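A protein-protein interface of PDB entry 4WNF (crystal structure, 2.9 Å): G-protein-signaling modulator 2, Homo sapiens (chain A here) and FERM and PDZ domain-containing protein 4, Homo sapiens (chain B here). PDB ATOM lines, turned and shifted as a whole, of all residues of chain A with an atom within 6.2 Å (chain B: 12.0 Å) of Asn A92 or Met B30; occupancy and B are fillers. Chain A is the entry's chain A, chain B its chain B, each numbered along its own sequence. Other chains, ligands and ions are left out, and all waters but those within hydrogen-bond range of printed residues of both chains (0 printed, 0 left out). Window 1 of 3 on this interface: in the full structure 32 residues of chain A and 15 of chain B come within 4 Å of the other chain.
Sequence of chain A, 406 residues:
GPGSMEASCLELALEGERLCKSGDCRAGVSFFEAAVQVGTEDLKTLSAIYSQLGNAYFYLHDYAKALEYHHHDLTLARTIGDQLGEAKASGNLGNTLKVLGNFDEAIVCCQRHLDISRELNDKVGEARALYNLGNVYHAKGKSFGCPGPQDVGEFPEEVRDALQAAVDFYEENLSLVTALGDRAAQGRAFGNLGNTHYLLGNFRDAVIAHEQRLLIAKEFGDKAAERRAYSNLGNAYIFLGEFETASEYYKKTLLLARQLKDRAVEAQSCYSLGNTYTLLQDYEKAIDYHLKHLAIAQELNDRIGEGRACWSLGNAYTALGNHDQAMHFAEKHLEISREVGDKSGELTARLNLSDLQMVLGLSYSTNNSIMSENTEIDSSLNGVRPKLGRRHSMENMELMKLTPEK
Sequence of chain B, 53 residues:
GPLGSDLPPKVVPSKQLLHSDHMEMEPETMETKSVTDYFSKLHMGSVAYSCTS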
ATOM      1  N   SER A  51      34.641  -3.402  10.682  1.00  0.00           N
ATOM      2  CA  SER A  51      34.055  -4.533  10.039  1.00  0.00           C
ATOM      3  C   SER A  51      34.660  -5.774  10.647  1.00  0.00           C
ATOM      4  O   SER A  51      33.947  -6.694  11.091  1.00  0.00           O
ATOM      5  CB  SER A  51      34.313  -4.486   8.553  1.00  0.00           C
ATOM      6  OG  SER A  51      33.326  -5.260   7.910  1.00  0.00           O
ATOM      7  N   GLY A  54      33.279  -6.436  13.864  1.00  0.00           N
ATOM      8  CA  GLY A  54      31.932  -6.937  13.734  1.00  0.00           C
ATOM      9  C   GLY A  54      31.895  -8.439  13.514  1.00  0.00           C
ATOM     10  O   GLY A  54      31.097  -9.143  14.129  1.00  0.00           O
ATOM     11  N   ASN A  55      32.759  -8.934  12.636  1.00  0.00           N
ATOM     12  CA  ASN A  55      32.745 -10.354  12.301  1.00  0.00           C
ATOM     13  C   ASN A  55      33.377 -11.158  13.431  1.00  0.00           C
ATOM     14  O   ASN A  55      32.810 -12.143  13.924  1.00  0.00           O
ATOM     15  CB  ASN A  55      33.472 -10.614  10.974  1.00  0.00           C
ATOM     16  CG  ASN A  55      32.739 -10.033   9.760  1.00  0.00           C
ATOM     17  OD1 ASN A  55      31.511  -9.847   9.767  1.00  0.00           O
ATOM     18  ND2 ASN A  55      33.496  -9.763   8.696  1.00  0.00           N
ATOM     19  N   PHE A  58      31.017 -11.477  15.827  1.00  0.00           N
ATOM     20  CA  PHE A  58      30.001 -12.387  15.308  1.00  0.00           C
ATOM     21  C   PHE A  58      30.413 -13.840  15.567  1.00  0.00           C
ATOM     22  O   PHE A  58      29.632 -14.635  16.104  1.00  0.00           O
ATOM     23  CB  PHE A  58      29.766 -12.174  13.810  1.00  0.00           C
ATOM     24  CG  PHE A  58      28.650 -13.021  13.241  1.00  0.00           C
ATOM     25  CD1 PHE A  58      28.857 -14.358  12.946  1.00  0.00           C
ATOM     26  CD2 PHE A  58      27.404 -12.481  13.003  1.00  0.00           C
ATOM     27  CE1 PHE A  58      27.845 -15.142  12.443  1.00  0.00           C
ATOM     28  CE2 PHE A  58      26.384 -13.262  12.497  1.00  0.00           C
ATOM     29  CZ  PHE A  58      26.605 -14.596  12.219  1.00  0.00           C
ATOM     30  N   HIS A  70      29.028  -3.224  12.938  1.00  0.00           N
ATOM     31  CA  HIS A  70      28.671  -3.154  11.523  1.00  0.00           C
ATOM     32  C   HIS A  70      27.785  -1.944  11.190  1.00  0.00           C
ATOM     33  O   HIS A  70      27.841  -1.368  10.104  1.00  0.00           O
ATOM     34  CB  HIS A  70      27.971  -4.419  11.135  1.00  0.00           C
ATOM     35  CG  HIS A  70      28.885  -5.592  11.031  1.00  0.00           C
ATOM     36  ND1 HIS A  70      28.631  -6.792  11.668  1.00  0.00           N
ATOM     37  CD2 HIS A  70      30.032  -5.764  10.334  1.00  0.00           C
ATOM     38  CE1 HIS A  70      29.587  -7.652  11.372  1.00  0.00           C
ATOM     39  NE2 HIS A  70      30.451  -7.052  10.566  1.00  0.00           N
ATOM     40  N   ASP A  73      30.160   0.658  10.735  1.00  0.00           N
ATOM     41  CA  ASP A  73      30.787   0.410   9.434  1.00  0.00           C
ATOM     42  C   ASP A  73      29.862   0.913   8.337  1.00  0.00           C
ATOM     43  O   ASP A  73      30.269   1.702   7.485  1.00  0.00           O
ATOM     44  CB  ASP A  73      31.079  -1.079   9.244  1.00  0.00           C
ATOM     45  CG  ASP A  73      31.782  -1.380   7.928  1.00  0.00           C
ATOM     46  OD1 ASP A  73      32.566  -0.525   7.465  1.00  0.00           O
ATOM     47  OD2 ASP A  73      31.563  -2.485   7.368  1.00  0.00           O
ATOM     48  N   ALA A  87      27.549  -1.909   0.642  1.00  0.00           N
ATOM     49  CA  ALA A  87      26.972  -3.204   0.278  1.00  0.00           C
ATOM     50  C   ALA A  87      27.357  -4.262   1.307  1.00  0.00           C
ATOM     51  O   ALA A  87      26.526  -5.029   1.813  1.00  0.00           O
ATOM     52  CB  ALA A  87      27.458  -3.626  -1.087  1.00  0.00           C
ATOM     53  N   LYS A  88      28.636  -4.284   1.632  1.00  0.00           N
ATOM     54  CA  LYS A  88      29.141  -5.282   2.540  1.00  0.00           C
ATOM     55  C   LYS A  88      28.580  -5.099   3.952  1.00  0.00           C
ATOM     56  O   LYS A  88      28.158  -6.064   4.615  1.00  0.00           O
ATOM     57  CB  LYS A  88      30.652  -5.196   2.603  1.00  0.00           C
ATOM     58  CG  LYS A  88      31.361  -5.289   1.259  1.00  0.00           C
ATOM     59  CD  LYS A  88      32.390  -6.411   1.260  1.00  0.00           C
ATOM     60  CE  LYS A  88      33.600  -6.117   0.396  1.00  0.00           C
ATOM     61  NZ  LYS A  88      34.545  -7.259   0.498  1.00  0.00           N
ATOM     62  N   ALA A  89      28.610  -3.865   4.436  1.00  0.00           N
ATOM     63  CA  ALA A  89      28.260  -3.641   5.826  1.00  0.00           C
ATOM     64  C   ALA A  89      26.806  -3.994   6.003  1.00  0.00           C
ATOM     65  O   ALA A  89      26.427  -4.609   7.002  1.00  0.00           O
ATOM     66  CB  ALA A  89      28.538  -2.212   6.239  1.00  0.00           C
ATOM     67  N   SER A  90      26.013  -3.632   4.995  1.00  0.00           N
ATOM     68  CA  SER A  90      24.615  -4.074   4.886  1.00  0.00           C
ATOM     69  C   SER A  90      24.499  -5.571   5.091  1.00  0.00           C
ATOM     70  O   SER A  90      23.740  -6.045   5.946  1.00  0.00           O
ATOM     71  CB  SER A  90      24.030  -3.722   3.507  1.00  0.00           C
ATOM     72  OG  SER A  90      23.481  -2.420   3.480  1.00  0.00           O
ATOM     73  N   GLY A  91      25.255  -6.317   4.295  1.00  0.00           N
ATOM     74  CA  GLY A  91      25.180  -7.765   4.371  1.00  0.00           C
ATOM     75  C   GLY A  91      25.402  -8.238   5.809  1.00  0.00           C
ATOM     76  O   GLY A  91      24.562  -8.958   6.413  1.00  0.00           O
ATOM     77  N   ASN A  92      26.522  -7.812   6.370  1.00  0.00           N
ATOM     78  CA  ASN A  92      26.893  -8.262   7.688  1.00  0.00           C
ATOM     79  C   ASN A  92      25.862  -7.855   8.725  1.00  0.00           C
ATOM     80  O   ASN A  92      25.443  -8.652   9.594  1.00  0.00           O
ATOM     81  CB  ASN A  92      28.259  -7.711   8.022  1.00  0.00           C
ATOM     82  CG  ASN A  92      29.338  -8.292   7.120  1.00  0.00           C
ATOM     83  OD1 ASN A  92      29.159  -9.371   6.535  1.00  0.00           O
ATOM     84  ND2 ASN A  92      30.458  -7.597   7.003  1.00  0.00           N
ATOM     85  N   LEU A  93      25.400  -6.624   8.628  1.00  0.00           N
ATOM     86  CA  LEU A  93      24.357  -6.194   9.559  1.00  0.00           C
ATOM     87  C   LEU A  93      23.102  -7.094   9.377  1.00  0.00           C
ATOM     88  O   LEU A  93      22.534  -7.641  10.352  1.00  0.00           O
ATOM     89  CB  LEU A  93      24.019  -4.745   9.269  1.00  0.00           C
ATOM     90  CG  LEU A  93      23.411  -3.885  10.362  1.00  0.00           C
ATOM     91  CD1 LEU A  93      24.317  -3.836  11.591  1.00  0.00           C
ATOM     92  CD2 LEU A  93      23.192  -2.487   9.754  1.00  0.00           C
ATOM     93  N   GLY A  94      22.712  -7.289   8.115  1.00  0.00           N
ATOM     94  CA  GLY A  94      21.559  -8.113   7.819  1.00  0.00           C
ATOM     95  C   GLY A  94      21.681  -9.479   8.472  1.00  0.00           C
ATOM     96  O   GLY A  94      20.777  -9.930   9.199  1.00  0.00           O
ATOM     97  N   ASN A  95      22.816 -10.127   8.252  1.00  0.00           N
ATOM     98  CA  ASN A  95      22.996 -11.487   8.785  1.00  0.00           C
ATOM     99  C   ASN A  95      22.893 -11.481  10.306  1.00  0.00           C
ATOM    100  O   ASN A  95      22.240 -12.350  10.900  1.00  0.00           O
ATOM    101  CB  ASN A  95      24.335 -12.079   8.328  1.00  0.00           C
ATOM    102  CG  ASN A  95      24.388 -12.333   6.798  1.00  0.00           C
ATOM    103  OD1 ASN A  95      23.341 -12.371   6.110  1.00  0.00           O
ATOM    104  ND2 ASN A  95      25.611 -12.519   6.261  1.00  0.00           N
ATOM    105  N   THR A  96      23.491 -10.462  10.926  1.00  0.00           N
ATOM    106  CA  THR A  96      23.484 -10.336  12.379  1.00  0.00           C
ATOM    107  C   THR A  96      22.086 -10.124  12.898  1.00  0.00           C
ATOM    108  O   THR A  96      21.646 -10.784  13.840  1.00  0.00           O
ATOM    109  CB  THR A  96      24.332  -9.137  12.836  1.00  0.00           C
ATOM    110  OG1 THR A  96      25.635  -9.214  12.230  1.00  0.00           O
ATOM    111  CG2 THR A  96      24.480  -9.148  14.378  1.00  0.00           C
ATOM    112  N   LEU A  97      21.381  -9.199  12.270  1.00  0.00           N
ATOM    113  CA  LEU A  97      19.973  -9.034  12.559  1.00  0.00           C
ATOM    114  C   LEU A  97      19.213 -10.356  12.411  1.00  0.00           C
ATOM    115  O   LEU A  97      18.299 -10.615  13.170  1.00  0.00           O
ATOM    116  CB  LEU A  97      19.383  -7.947  11.675  1.00  0.00           C
ATOM    117  CG  LEU A  97      19.925  -6.562  12.049  1.00  0.00           C
ATOM    118  CD1 LEU A  97      19.712  -5.575  10.914  1.00  0.00           C
ATOM    119  CD2 LEU A  97      19.281  -6.048  13.325  1.00  0.00           C
ATOM    120  N   HIS A 113      22.211  -5.042   0.071  1.00  0.00           N
ATOM    121  CA  HIS A 113      23.465  -5.648  -0.313  1.00  0.00           C
ATOM    122  C   HIS A 113      23.306  -6.160  -1.738  1.00  0.00           C
ATOM    123  O   HIS A 113      24.138  -5.898  -2.614  1.00  0.00           O
ATOM    124  CB  HIS A 113      23.737  -6.773   0.674  1.00  0.00           C
ATOM    125  CG  HIS A 113      24.943  -7.592   0.373  1.00  0.00           C
ATOM    126  ND1 HIS A 113      25.185  -8.796   1.006  1.00  0.00           N
ATOM    127  CD2 HIS A 113      25.968  -7.399  -0.487  1.00  0.00           C
ATOM    128  CE1 HIS A 113      26.321  -9.299   0.560  1.00  0.00           C
ATOM    129  NE2 HIS A 113      26.812  -8.476  -0.351  1.00  0.00           N
ATOM    130  N   ARG A 128      26.239 -14.061  -2.961  1.00  0.00           N
ATOM    131  CA  ARG A 128      26.250 -14.148  -1.491  1.00  0.00           C
ATOM    132  C   ARG A 128      24.995 -13.540  -0.878  1.00  0.00           C
ATOM    133  O   ARG A 128      24.392 -14.105   0.051  1.00  0.00           O
ATOM    134  CB  ARG A 128      27.416 -13.383  -0.908  1.00  0.00           C
ATOM    135  CG  ARG A 128      28.743 -13.628  -1.576  1.00  0.00           C
ATOM    136  CD  ARG A 128      29.705 -14.357  -0.675  1.00  0.00           C
ATOM    137  NE  ARG A 128      30.965 -13.635  -0.562  1.00  0.00           N
ATOM    138  CZ  ARG A 128      31.867 -13.872   0.383  1.00  0.00           C
ATOM    139  NH1 ARG A 128      32.985 -13.164   0.417  1.00  0.00           N
ATOM    140  NH2 ARG A 128      31.660 -14.817   1.302  1.00  0.00           N
ATOM    141  N   ASN A 132      22.347 -15.066   1.581  1.00  0.00           N
ATOM    142  CA  ASN A 132      22.011 -14.429   2.830  1.00  0.00           C
ATOM    143  C   ASN A 132      20.514 -14.224   2.959  1.00  0.00           C
ATOM    144  O   ASN A 132      19.923 -14.512   4.009  1.00  0.00           O
ATOM    145  CB  ASN A 132      22.709 -13.099   2.928  1.00  0.00           C
ATOM    146  CG  ASN A 132      24.178 -13.252   3.135  1.00  0.00           C
ATOM    147  OD1 ASN A 132      24.630 -14.321   3.514  1.00  0.00           O
ATOM    148  ND2 ASN A 132      24.939 -12.190   2.901  1.00  0.00           N
ATOM    149  N   GLU B  26      23.780 -24.797   7.396  1.00  0.00           N
ATOM    150  CA  GLU B  26      25.092 -24.401   6.922  1.00  0.00           C
ATOM    151  C   GLU B  26      25.458 -23.057   7.546  1.00  0.00           C
ATOM    152  O   GLU B  26      24.576 -22.267   7.877  1.00  0.00           O
ATOM    153  CB  GLU B  26      25.098 -24.333   5.390  1.00  0.00           C
ATOM    154  CG  GLU B  26      24.641 -25.622   4.676  1.00  0.00           C
ATOM    155  CD  GLU B  26      25.549 -26.841   4.916  1.00  0.00           C
ATOM    156  OE1 GLU B  26      26.778 -26.718   4.694  1.00  0.00           O
ATOM    157  OE2 GLU B  26      25.036 -27.935   5.299  1.00  0.00           O
ATOM    158  N   PRO B  27      26.758 -22.787   7.706  1.00  0.00           N
ATOM    159  CA  PRO B  27      27.163 -21.522   8.308  1.00  0.00           C
ATOM    160  C   PRO B  27      26.805 -20.320   7.448  1.00  0.00           C
ATOM    161  O   PRO B  27      26.465 -20.471   6.280  1.00  0.00           O
ATOM    162  CB  PRO B  27      28.684 -21.651   8.383  1.00  0.00           C
ATOM    163  CG  PRO B  27      29.034 -22.533   7.225  1.00  0.00           C
ATOM    164  CD  PRO B  27      27.905 -23.520   7.137  1.00  0.00           C
ATOM    165  N   GLU B  28      26.887 -19.130   8.028  1.00  0.00           N
ATOM    166  CA  GLU B  28      26.669 -17.902   7.274  1.00  0.00           C
ATOM    167  C   GLU B  28      27.964 -17.471   6.619  1.00  0.00           C
ATOM    168  O   GLU B  28      29.054 -17.792   7.083  1.00  0.00           O
ATOM    169  CB  GLU B  28      26.206 -16.757   8.177  1.00  0.00           C
ATOM    170  CG  GLU B  28      24.826 -16.899   8.800  1.00  0.00           C
ATOM    171  CD  GLU B  28      24.825 -17.553  10.185  1.00  0.00           C
ATOM    172  OE1 GLU B  28      23.732 -17.971  10.635  1.00  0.00           O
ATOM    173  OE2 GLU B  28      25.895 -17.645  10.834  1.00  0.00           O
ATOM    174  N   THR B  29      27.817 -16.733   5.531  1.00  0.00           N
ATOM    175  CA  THR B  29      28.909 -16.013   4.936  1.00  0.00           C
ATOM    176  C   THR B  29      28.861 -14.577   5.416  1.00  0.00           C
ATOM    177  O   THR B  29      27.822 -13.926   5.357  1.00  0.00           O
ATOM    178  CB  THR B  29      28.782 -15.969   3.403  1.00  0.00           C
ATOM    179  OG1 THR B  29      27.528 -15.380   3.023  1.00  0.00           O
ATOM    180  CG2 THR B  29      28.874 -17.355   2.820  1.00  0.00           C
ATOM    181  N   MET B  30      29.990 -14.052   5.843  1.00  0.00           N
ATOM    182  CA  MET B  30      30.071 -12.632   6.104  1.00  0.00           C
ATOM    183  C   MET B  30      31.063 -12.034   5.121  1.00  0.00           C
ATOM    184  O   MET B  30      32.140 -12.576   4.940  1.00  0.00           O
ATOM    185  CB  MET B  30      30.527 -12.387   7.541  1.00  0.00           C
ATOM    186  CG  MET B  30      29.727 -13.162   8.591  1.00  0.00           C
ATOM    187  SD  MET B  30      28.076 -12.538   8.997  1.00  0.00           S
ATOM    188  CE  MET B  30      28.494 -10.935   9.660  1.00  0.00           C
ATOM    189  N   GLU B  31      30.705 -10.926   4.478  1.00  0.00           N
ATOM    190  CA  GLU B  31      31.657 -10.233   3.610  1.00  0.00           C
ATOM    191  C   GLU B  31      32.722  -9.624   4.506  1.00  0.00           C
ATOM    192  O   GLU B  31      32.454  -9.364   5.678  1.00  0.00           O
ATOM    193  CB  GLU B  31      30.998  -9.141   2.772  1.00  0.00           C
ATOM    194  CG  GLU B  31      29.612  -9.472   2.237  1.00  0.00           C
ATOM    195  CD  GLU B  31      29.500 -10.873   1.673  1.00  0.00           C
ATOM    196  OE1 GLU B  31      28.656 -11.681   2.200  1.00  0.00           O
ATOM    197  OE2 GLU B  31      30.264 -11.153   0.715  1.00  0.00           O
ATOM    198  N   THR B  32      33.925  -9.417   3.964  1.00  0.00           N
ATOM    199  CA  THR B  32      35.093  -9.073   4.784  1.00  0.00           C
ATOM    200  C   THR B  32      35.951  -7.953   4.185  1.00  0.00           C
ATOM    201  O   THR B  32      36.376  -8.015   3.053  1.00  0.00           O
ATOM    202  CB  THR B  32      36.013 -10.303   5.010  1.00  0.00           C
ATOM    203  OG1 THR B  32      36.613 -10.675   3.776  1.00  0.00           O
ATOM    204  CG2 THR B  32      35.247 -11.505   5.568  1.00  0.00           C
ATOM    205  N   LYS B  33      36.248  -6.949   4.985  1.00  0.00           N
ATOM    206  CA  LYS B  33      37.054  -5.848   4.529  1.00  0.00           C
ATOM    207  C   LYS B  33      38.446  -5.948   5.124  1.00  0.00           C
ATOM    208  O   LYS B  33      38.613  -6.394   6.259  1.00  0.00           O
ATOM    209  CB  LYS B  33      36.416  -4.521   4.966  1.00  0.00           C
ATOM    210  CG  LYS B  33      34.931  -4.370   4.652  1.00  0.00           C
ATOM    211  CD  LYS B  33      34.570  -2.903   4.596  1.00  0.00           C
ATOM    212  CE  LYS B  33      33.082  -2.662   4.508  1.00  0.00           C
ATOM    213  NZ  LYS B  33      32.838  -1.193   4.572  1.00  0.00           N
ATOM    214  N   SER B  34      39.438  -5.482   4.379  1.00  0.00           N
ATOM    215  CA  SER B  34      40.808  -5.477   4.854  1.00  0.00           C
ATOM    216  C   SER B  34      41.424  -4.078   4.843  1.00  0.00           C
ATOM    217  O   SER B  34      41.097  -3.242   3.999  1.00  0.00           O
ATOM    218  CB  SER B  34      41.645  -6.403   3.987  1.00  0.00           C
ATOM    219  OG  SER B  34      43.007  -6.259   4.304  1.00  0.00           O
ATOM    220  N   ASP B  37      43.565  -3.445   1.682  1.00  0.00           N
ATOM    221  CA  ASP B  37      42.906  -2.864   0.516  1.00  0.00           C
ATOM    222  C   ASP B  37      43.539  -1.529   0.099  1.00  0.00           C
ATOM    223  O   ASP B  37      43.521  -1.177  -1.085  1.00  0.00           O
ATOM    224  CB  ASP B  37      41.407  -2.676   0.790  1.00  0.00           C
ATOM    225  CG  ASP B  37      40.658  -4.007   0.934  1.00  0.00           C
ATOM    226  OD1 ASP B  37      41.087  -5.015   0.326  1.00  0.00           O
ATOM    227  OD2 ASP B  37      39.628  -4.036   1.649  1.00  0.00           O
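The side-chain hydroxyl of Ser A51 lies within hydrogen-bond range of the side-chain carboxylate of Asp A73.
The side-chain amide nitrogen of Asn A132 sits close to the backbone carbonyl oxygen of Arg A128, at 3.5 Å.
OD1 of Asn A132 sits at hydrogen-bond distance from ND2 of Asn A95.
The backbone carbonyl oxygen of Asn A92 lies within hydrogen-bond range of the side-chain hydroxyl of Thr A96, at 2.7 Å.
NE2 of His A70 is in hydrogen-bond range of OD1 of Asn A55 (3.1 Å).
Of chain B, only Lys B33 comes within 4 Å of Ser A51.
Printed residues of chain B within 4 Å of Asn A55: Met B30 (3.2 Å), Glu B31 (3.2 Å) and Thr B32 (3.99 Å).
Phe A58 touches just these residues of chain B: Glu B28 and Met B30.
Of chain B, only Met B30 comes within 4 Å of His A70.
Printed residues of chain B within 4 Å of Lys A88: Glu B31 (3.4 Å), Thr B32 (3.2 Å) and Lys B33 (3.99 Å).
No residue of chain B comes within 4 Å of Ala A89.
Asn A92 touches just these residues of chain B: Met B30 (3.4 Å) and Glu B31 (3.0 Å).
No residue of chain B comes within 4 Å of Leu A93.
Gly A94 touches none of the printed residues of chain B.
Printed residues of chain B within 4 Å of Asn A95: Thr B29 (2.8 Å) and Met B30 (3.7 Å).
No residue of chain B comes within 4 Å of Thr A96.
Of the printed residues of chain A, Glu B28 touches Phe A58.
Printed residues of chain A within 4 Å of Thr B29: Asn A95 (2.8 Å), Arg A128 (3.7 Å) and Asn A132 (3.1 Å).
Met B30 touches just these residues of chain A: Asn A55 (3.2 Å), Phe A58 (3.8 Å), His A70 (3.9 Å), Asn A92 (3.4 Å) and Asn A95 (3.7 Å).
Printed residues of chain A within 4 Å of Glu B31: Asn A55, Lys A88, Asn A92, His A113, Arg A128 and Asn A132.
The nearest printed residue of chain A that does not touch Thr B29 is Asn A92 (4.9 Å).
Of the 10 printed residues of chain B, 6 touch a printed residue of chain A.
Of the 20 printed residues of chain A, 11 touch a printed residue of chain B.
Among the printed residues, 20 pairs touch across the chains.
Among the printed residues, Asp or Glu carboxylates within 4 Å of a Lys or Arg side-chain nitrogen of the other chain: Asp A73 with Lys B33 and Arg A128 with Glu B31.
O of Thr B29 sits at hydrogen-bond distance from ND2 of Asn A95, at 2.8 Å.
The side-chain amide nitrogen (ND2) of Asn A92 sits at hydrogen-bond distance from the backbone carbonyl oxygen (O) of Glu B31, 3.0 Å away.
OD1 of Asp A73 lies within salt-bridge range of NZ of Lys B33 (3.0 Å).
The side-chain amino group of Lys A88 sits at hydrogen-bond distance from the backbone carbonyl oxygen of Thr B32, at 3.2 Å.
The side-chain carboxylate (OE2) of Glu B31 is in salt-bridge range of the guanidinium group (NE) of Arg A128 (2.9 Å).
The side-chain amide oxygen of Asn A132 is in hydrogen-bond range of the side-chain hydroxyl of Thr B29 (3.1 Å).
O of Glu B31 lies within hydrogen-bond range of ND2 of Asn A55, at 3.2 Å.
SD of Met B30 lies within hydrogen-bond range of ND2 of Asn A95, 3.7 Å away.
CG of Lys B33 touches OG of Ser A51, at 3.7 Å.
CE of Met B30 touches OD1 of Asn A55, 3.2 Å away.
Asn A55 touches Thr B32 (ND2 to CG2, 3.99 Å).
Phe A58 touches Glu B28 (CZ to OE2, 3.4 Å).
His A70 touches Met B30.
CE of Lys B33 touches CB of Lys A88, 3.99 Å away.
Met B30 touches Asn A92 (CA to OD1, 3.4 Å).
His A113 touches Glu B31 (CE1 to CG, 3.7 Å).
CB of Thr B29 touches NH2 of Arg A128, 3.7 Å away.
Asn A132 touches Glu B31 (ND2 to OE1, 3.8 Å).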
